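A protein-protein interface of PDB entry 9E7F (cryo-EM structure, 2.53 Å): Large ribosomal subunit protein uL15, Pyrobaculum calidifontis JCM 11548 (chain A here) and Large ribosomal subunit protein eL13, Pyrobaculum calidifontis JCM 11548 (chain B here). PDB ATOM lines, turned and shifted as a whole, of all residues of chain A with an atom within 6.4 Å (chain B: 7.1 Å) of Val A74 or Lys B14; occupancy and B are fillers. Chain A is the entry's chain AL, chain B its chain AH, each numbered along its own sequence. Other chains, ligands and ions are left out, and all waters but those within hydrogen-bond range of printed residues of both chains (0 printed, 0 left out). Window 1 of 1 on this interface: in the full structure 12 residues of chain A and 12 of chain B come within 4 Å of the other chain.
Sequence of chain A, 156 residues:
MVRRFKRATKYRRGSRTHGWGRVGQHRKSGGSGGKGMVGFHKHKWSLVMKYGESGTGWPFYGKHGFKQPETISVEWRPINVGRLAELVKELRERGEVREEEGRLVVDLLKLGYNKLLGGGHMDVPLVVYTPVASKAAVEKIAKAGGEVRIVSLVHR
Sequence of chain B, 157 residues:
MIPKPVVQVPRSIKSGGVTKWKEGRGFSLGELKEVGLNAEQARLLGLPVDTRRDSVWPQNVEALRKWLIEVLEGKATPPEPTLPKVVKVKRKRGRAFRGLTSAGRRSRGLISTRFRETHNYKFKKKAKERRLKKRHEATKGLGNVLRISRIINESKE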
ATOM      1  N   PRO A  69      -1.524  18.858  -9.906  1.00  0.00           N
ATOM      2  CA  PRO A  69      -1.099  18.132  -8.705  1.00  0.00           C
ATOM      3  C   PRO A  69      -2.234  17.946  -7.709  1.00  0.00           C
ATOM      4  O   PRO A  69      -3.022  18.858  -7.456  1.00  0.00           O
ATOM      5  CB  PRO A  69       0.016  19.015  -8.137  1.00  0.00           C
ATOM      6  CG  PRO A  69       0.434  19.895  -9.252  1.00  0.00           C
ATOM      7  CD  PRO A  69      -0.764  20.101 -10.100  1.00  0.00           C
ATOM      8  N   GLU A  70      -2.319  16.738  -7.153  1.00  0.00           N
ATOM      9  CA  GLU A  70      -3.411  16.399  -6.250  1.00  0.00           C
ATOM     10  C   GLU A  70      -3.290  17.095  -4.906  1.00  0.00           C
ATOM     11  O   GLU A  70      -4.284  17.191  -4.182  1.00  0.00           O
ATOM     12  CB  GLU A  70      -3.472  14.885  -6.047  1.00  0.00           C
ATOM     13  CG  GLU A  70      -2.110  14.225  -5.922  1.00  0.00           C
ATOM     14  CD  GLU A  70      -2.196  12.714  -5.836  1.00  0.00           C
ATOM     15  OE1 GLU A  70      -3.186  12.142  -6.337  1.00  0.00           O
ATOM     16  OE2 GLU A  70      -1.266  12.097  -5.276  1.00  0.00           O
ATOM     17  N   THR A  71      -2.104  17.582  -4.558  1.00  0.00           N
ATOM     18  CA  THR A  71      -1.899  18.236  -3.276  1.00  0.00           C
ATOM     19  C   THR A  71      -2.345  19.691  -3.268  1.00  0.00           C
ATOM     20  O   THR A  71      -2.449  20.280  -2.189  1.00  0.00           O
ATOM     21  CB  THR A  71      -0.425  18.145  -2.884  1.00  0.00           C
ATOM     22  OG1 THR A  71       0.387  18.403  -4.035  1.00  0.00           O
ATOM     23  CG2 THR A  71      -0.111  16.757  -2.346  1.00  0.00           C
ATOM     24  N   ILE A  72      -2.609  20.284  -4.430  1.00  0.00           N
ATOM     25  CA  ILE A  72      -3.077  21.660  -4.518  1.00  0.00           C
ATOM     26  C   ILE A  72      -4.474  21.762  -5.098  1.00  0.00           C
ATOM     27  O   ILE A  72      -5.019  22.865  -5.178  1.00  0.00           O
ATOM     28  CB  ILE A  72      -2.100  22.536  -5.329  1.00  0.00           C
ATOM     29  CG1 ILE A  72      -2.007  22.034  -6.771  1.00  0.00           C
ATOM     30  CG2 ILE A  72      -0.734  22.550  -4.670  1.00  0.00           C
ATOM     31  CD1 ILE A  72      -1.478  23.050  -7.754  1.00  0.00           C
ATOM     32  N   SER A  73      -5.071  20.648  -5.502  1.00  0.00           N
ATOM     33  CA  SER A  73      -6.411  20.619  -6.065  1.00  0.00           C
ATOM     34  C   SER A  73      -7.414  20.119  -5.033  1.00  0.00           C
ATOM     35  O   SER A  73      -7.059  19.484  -4.040  1.00  0.00           O
ATOM     36  CB  SER A  73      -6.457  19.734  -7.311  1.00  0.00           C
ATOM     37  OG  SER A  73      -5.352  19.985  -8.160  1.00  0.00           O
ATOM     38  N   VAL A  74      -8.677  20.411  -5.287  1.00  0.00           N
ATOM     39  CA  VAL A  74      -9.763  20.051  -4.386  1.00  0.00           C
ATOM     40  C   VAL A  74     -10.348  18.711  -4.805  1.00  0.00           C
ATOM     41  O   VAL A  74     -10.538  18.440  -5.995  1.00  0.00           O
ATOM     42  CB  VAL A  74     -10.846  21.144  -4.369  1.00  0.00           C
ATOM     43  CG1 VAL A  74     -12.036  20.690  -3.556  1.00  0.00           C
ATOM     44  CG2 VAL A  74     -10.282  22.424  -3.810  1.00  0.00           C
ATOM     45  N   GLU A  75     -10.618  17.864  -3.817  1.00  0.00           N
ATOM     46  CA  GLU A  75     -11.358  16.622  -4.019  1.00  0.00           C
ATOM     47  C   GLU A  75     -12.837  16.961  -3.878  1.00  0.00           C
ATOM     48  O   GLU A  75     -13.275  17.458  -2.837  1.00  0.00           O
ATOM     49  CB  GLU A  75     -10.897  15.564  -3.021  1.00  0.00           C
ATOM     50  CG  GLU A  75     -11.697  14.275  -3.022  1.00  0.00           C
ATOM     51  CD  GLU A  75     -12.751  14.232  -1.935  1.00  0.00           C
ATOM     52  OE1 GLU A  75     -13.336  13.152  -1.717  1.00  0.00           O
ATOM     53  OE2 GLU A  75     -12.985  15.271  -1.286  1.00  0.00           O
ATOM     54  N   TRP A  76     -13.607  16.713  -4.935  1.00  0.00           N
ATOM     55  CA  TRP A  76     -14.991  17.164  -4.980  1.00  0.00           C
ATOM     56  C   TRP A  76     -15.947  16.050  -4.581  1.00  0.00           C
ATOM     57  O   TRP A  76     -15.837  14.917  -5.059  1.00  0.00           O
ATOM     58  CB  TRP A  76     -15.334  17.685  -6.371  1.00  0.00           C
ATOM     59  CG  TRP A  76     -14.672  18.972  -6.667  1.00  0.00           C
ATOM     60  CD1 TRP A  76     -13.670  19.190  -7.558  1.00  0.00           C
ATOM     61  CD2 TRP A  76     -14.952  20.235  -6.060  1.00  0.00           C
ATOM     62  NE1 TRP A  76     -13.308  20.513  -7.548  1.00  0.00           N
ATOM     63  CE2 TRP A  76     -14.081  21.175  -6.634  1.00  0.00           C
ATOM     64  CE3 TRP A  76     -15.855  20.660  -5.086  1.00  0.00           C
ATOM     65  CZ2 TRP A  76     -14.088  22.513  -6.270  1.00  0.00           C
ATOM     66  CZ3 TRP A  76     -15.859  21.987  -4.726  1.00  0.00           C
ATOM     67  CH2 TRP A  76     -14.982  22.899  -5.317  1.00  0.00           C
ATOM     68  N   ASN A 114     -19.161  18.833  -0.503  1.00  0.00           N
ATOM     69  CA  ASN A 114     -18.618  20.160  -0.741  1.00  0.00           C
ATOM     70  C   ASN A 114     -19.245  20.878  -1.926  1.00  0.00           C
ATOM     71  O   ASN A 114     -18.978  22.068  -2.109  1.00  0.00           O
ATOM     72  CB  ASN A 114     -17.100  20.091  -0.939  1.00  0.00           C
ATOM     73  CG  ASN A 114     -16.685  18.952  -1.830  1.00  0.00           C
ATOM     74  OD1 ASN A 114     -17.493  18.416  -2.583  1.00  0.00           O
ATOM     75  ND2 ASN A 114     -15.416  18.575  -1.756  1.00  0.00           N
ATOM     76  N   LEU A 153     -14.101  29.119   2.136  1.00  0.00           N
ATOM     77  CA  LEU A 153     -13.302  28.274   3.018  1.00  0.00           C
ATOM     78  C   LEU A 153     -12.262  29.058   3.812  1.00  0.00           C
ATOM     79  O   LEU A 153     -12.447  30.236   4.106  1.00  0.00           O
ATOM     80  CB  LEU A 153     -12.618  27.181   2.197  1.00  0.00           C
ATOM     81  CG  LEU A 153     -13.592  26.206   1.536  1.00  0.00           C
ATOM     82  CD1 LEU A 153     -12.874  25.293   0.563  1.00  0.00           C
ATOM     83  CD2 LEU A 153     -14.339  25.407   2.588  1.00  0.00           C
ATOM     84  N   ARG B  11      -6.845  20.623   8.249  1.00  0.00           N
ATOM     85  CA  ARG B  11      -7.746  20.733   7.107  1.00  0.00           C
ATOM     86  C   ARG B  11      -6.929  20.974   5.846  1.00  0.00           C
ATOM     87  O   ARG B  11      -6.328  22.038   5.682  1.00  0.00           O
ATOM     88  CB  ARG B  11      -8.749  21.857   7.339  1.00  0.00           C
ATOM     89  CG  ARG B  11      -9.802  21.983   6.268  1.00  0.00           C
ATOM     90  CD  ARG B  11     -10.800  23.070   6.605  1.00  0.00           C
ATOM     91  NE  ARG B  11     -10.177  24.384   6.675  1.00  0.00           N
ATOM     92  CZ  ARG B  11     -10.829  25.507   6.937  1.00  0.00           C
ATOM     93  NH1 ARG B  11     -12.137  25.516   7.133  1.00  0.00           N
ATOM     94  NH2 ARG B  11     -10.156  26.650   6.996  1.00  0.00           N
ATOM     95  N   SER B  12      -6.913  19.996   4.954  1.00  0.00           N
ATOM     96  CA  SER B  12      -6.106  20.057   3.749  1.00  0.00           C
ATOM     97  C   SER B  12      -6.849  20.765   2.623  1.00  0.00           C
ATOM     98  O   SER B  12      -8.067  20.946   2.661  1.00  0.00           O
ATOM     99  CB  SER B  12      -5.708  18.654   3.306  1.00  0.00           C
ATOM    100  OG  SER B  12      -6.831  17.792   3.287  1.00  0.00           O
ATOM    101  N   ILE B  13      -6.084  21.180   1.613  1.00  0.00           N
ATOM    102  CA  ILE B  13      -6.684  21.789   0.433  1.00  0.00           C
ATOM    103  C   ILE B  13      -7.499  20.761  -0.334  1.00  0.00           C
ATOM    104  O   ILE B  13      -8.548  21.076  -0.908  1.00  0.00           O
ATOM    105  CB  ILE B  13      -5.596  22.425  -0.448  1.00  0.00           C
ATOM    106  CG1 ILE B  13      -5.332  23.861  -0.011  1.00  0.00           C
ATOM    107  CG2 ILE B  13      -6.004  22.391  -1.904  1.00  0.00           C
ATOM    108  CD1 ILE B  13      -4.008  24.390  -0.482  1.00  0.00           C
ATOM    109  N   LYS B  14      -7.033  19.512  -0.348  1.00  0.00           N
ATOM    110  CA  LYS B  14      -7.750  18.439  -1.026  1.00  0.00           C
ATOM    111  C   LYS B  14      -9.098  18.159  -0.374  1.00  0.00           C
ATOM    112  O   LYS B  14     -10.029  17.709  -1.050  1.00  0.00           O
ATOM    113  CB  LYS B  14      -6.878  17.182  -1.036  1.00  0.00           C
ATOM    114  CG  LYS B  14      -7.239  16.166   0.025  1.00  0.00           C
ATOM    115  CD  LYS B  14      -6.813  14.760  -0.347  1.00  0.00           C
ATOM    116  CE  LYS B  14      -5.307  14.674  -0.504  1.00  0.00           C
ATOM    117  NZ  LYS B  14      -4.792  13.328  -0.126  1.00  0.00           N
ATOM    118  N   SER B  15      -9.227  18.438   0.926  1.00  0.00           N
ATOM    119  CA  SER B  15     -10.448  18.104   1.653  1.00  0.00           C
ATOM    120  C   SER B  15     -11.636  18.939   1.193  1.00  0.00           C
ATOM    121  O   SER B  15     -12.778  18.473   1.253  1.00  0.00           O
ATOM    122  CB  SER B  15     -10.224  18.289   3.151  1.00  0.00           C
ATOM    123  OG  SER B  15     -10.552  19.606   3.555  1.00  0.00           O
ATOM    124  N   GLY B  16     -11.394  20.167   0.748  1.00  0.00           N
ATOM    125  CA  GLY B  16     -12.475  21.029   0.318  1.00  0.00           C
ATOM    126  C   GLY B  16     -13.313  21.612   1.430  1.00  0.00           C
ATOM    127  O   GLY B  16     -14.446  22.032   1.182  1.00  0.00           O
ATOM    128  N   GLY B  17     -12.798  21.655   2.652  1.00  0.00           N
ATOM    129  CA  GLY B  17     -13.529  22.217   3.764  1.00  0.00           C
ATOM    130  C   GLY B  17     -14.226  21.219   4.658  1.00  0.00           C
ATOM    131  O   GLY B  17     -14.945  21.636   5.570  1.00  0.00           O
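Printed residues of chain B that touch a printed residue of chain A: Ile B13, Lys B14, Gly B16 and Gly B17. Of the 10 printed residues of chain A, 6 touch a printed residue of chain B. Printed residues of chain A that touch a printed residue of chain B: Ile A72, Ser A73, Val A74, Glu A75, Asn A114 and Leu A153. Hydrophobic or aromatic side chains of chain A that line the printed part of chain B: Val A74 and Leu A153. Among the printed residues, no Asp or Glu carboxylate lies within 4 Å of a Lys or Arg side-chain nitrogen of the other chain.
Ile B13 touches Ile A72. Ile B13 touches Ser A73 (CG2 to O, 3.8 Å). Ser A73 touches Lys B14. CG2 of Val A74 touches O of Ile B13, at 3.6 Å. Val A74 touches Lys B14 (C to O, 3.9 Å). Val A74 touches Gly B16 (CG1 to CA, 3.9 Å). CB of Asn A114 touches O of Gly B16, 3.9 Å away. Leu A153 touches Gly B16. CD2 of Leu A153 touches CA of Gly B17, 3.5 Å away.
The backbone carbonyl oxygen of Lys B14 is in hydrogen-bond range of the backbone NH of Glu A75, at 2.8 Å.
Of the printed residues of chain B, Val A74 touches Ile B13 (3.6 Å), Lys B14 (3.9 Å) and Gly B16 (3.9 Å). Lys B14 touches just these residues of chain A: Ser A73, Val A74 and Glu A75. Printed residues of chain B within 4 Å of Asn A114: Gly B16 (3.9 Å). Of the printed residues of chain B, Ile A72 touches Ile B13 (3.5 Å). Of the printed residues of chain A, Gly B17 touches Leu A153. Printed residues of chain B within 4 Å of Glu A75: Lys B14 (2.8 Å). Of the printed residues of chain B, Ser A73 touches Ile B13 (3.8 Å) and Lys B14 (3.3 Å). Glu A70 touches none of the printed residues of chain B. The nearest printed residue of chain B that does not touch Asn A114 is Ser B15 (4.003 Å).
The side-chain hydroxyl (OG) of Ser B15 lies within hydrogen-bond range of the backbone NH (N) of Gly B17 (3.2 Å). The side-chain amide nitrogen of Asn A114 lies within hydrogen-bond range of the backbone carbonyl oxygen of Glu A75 (2.6 Å). The backbone carbonyl oxygen (O) of Pro A69 is in hydrogen-bond range of the side-chain hydroxyl (OG) of Ser A73.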
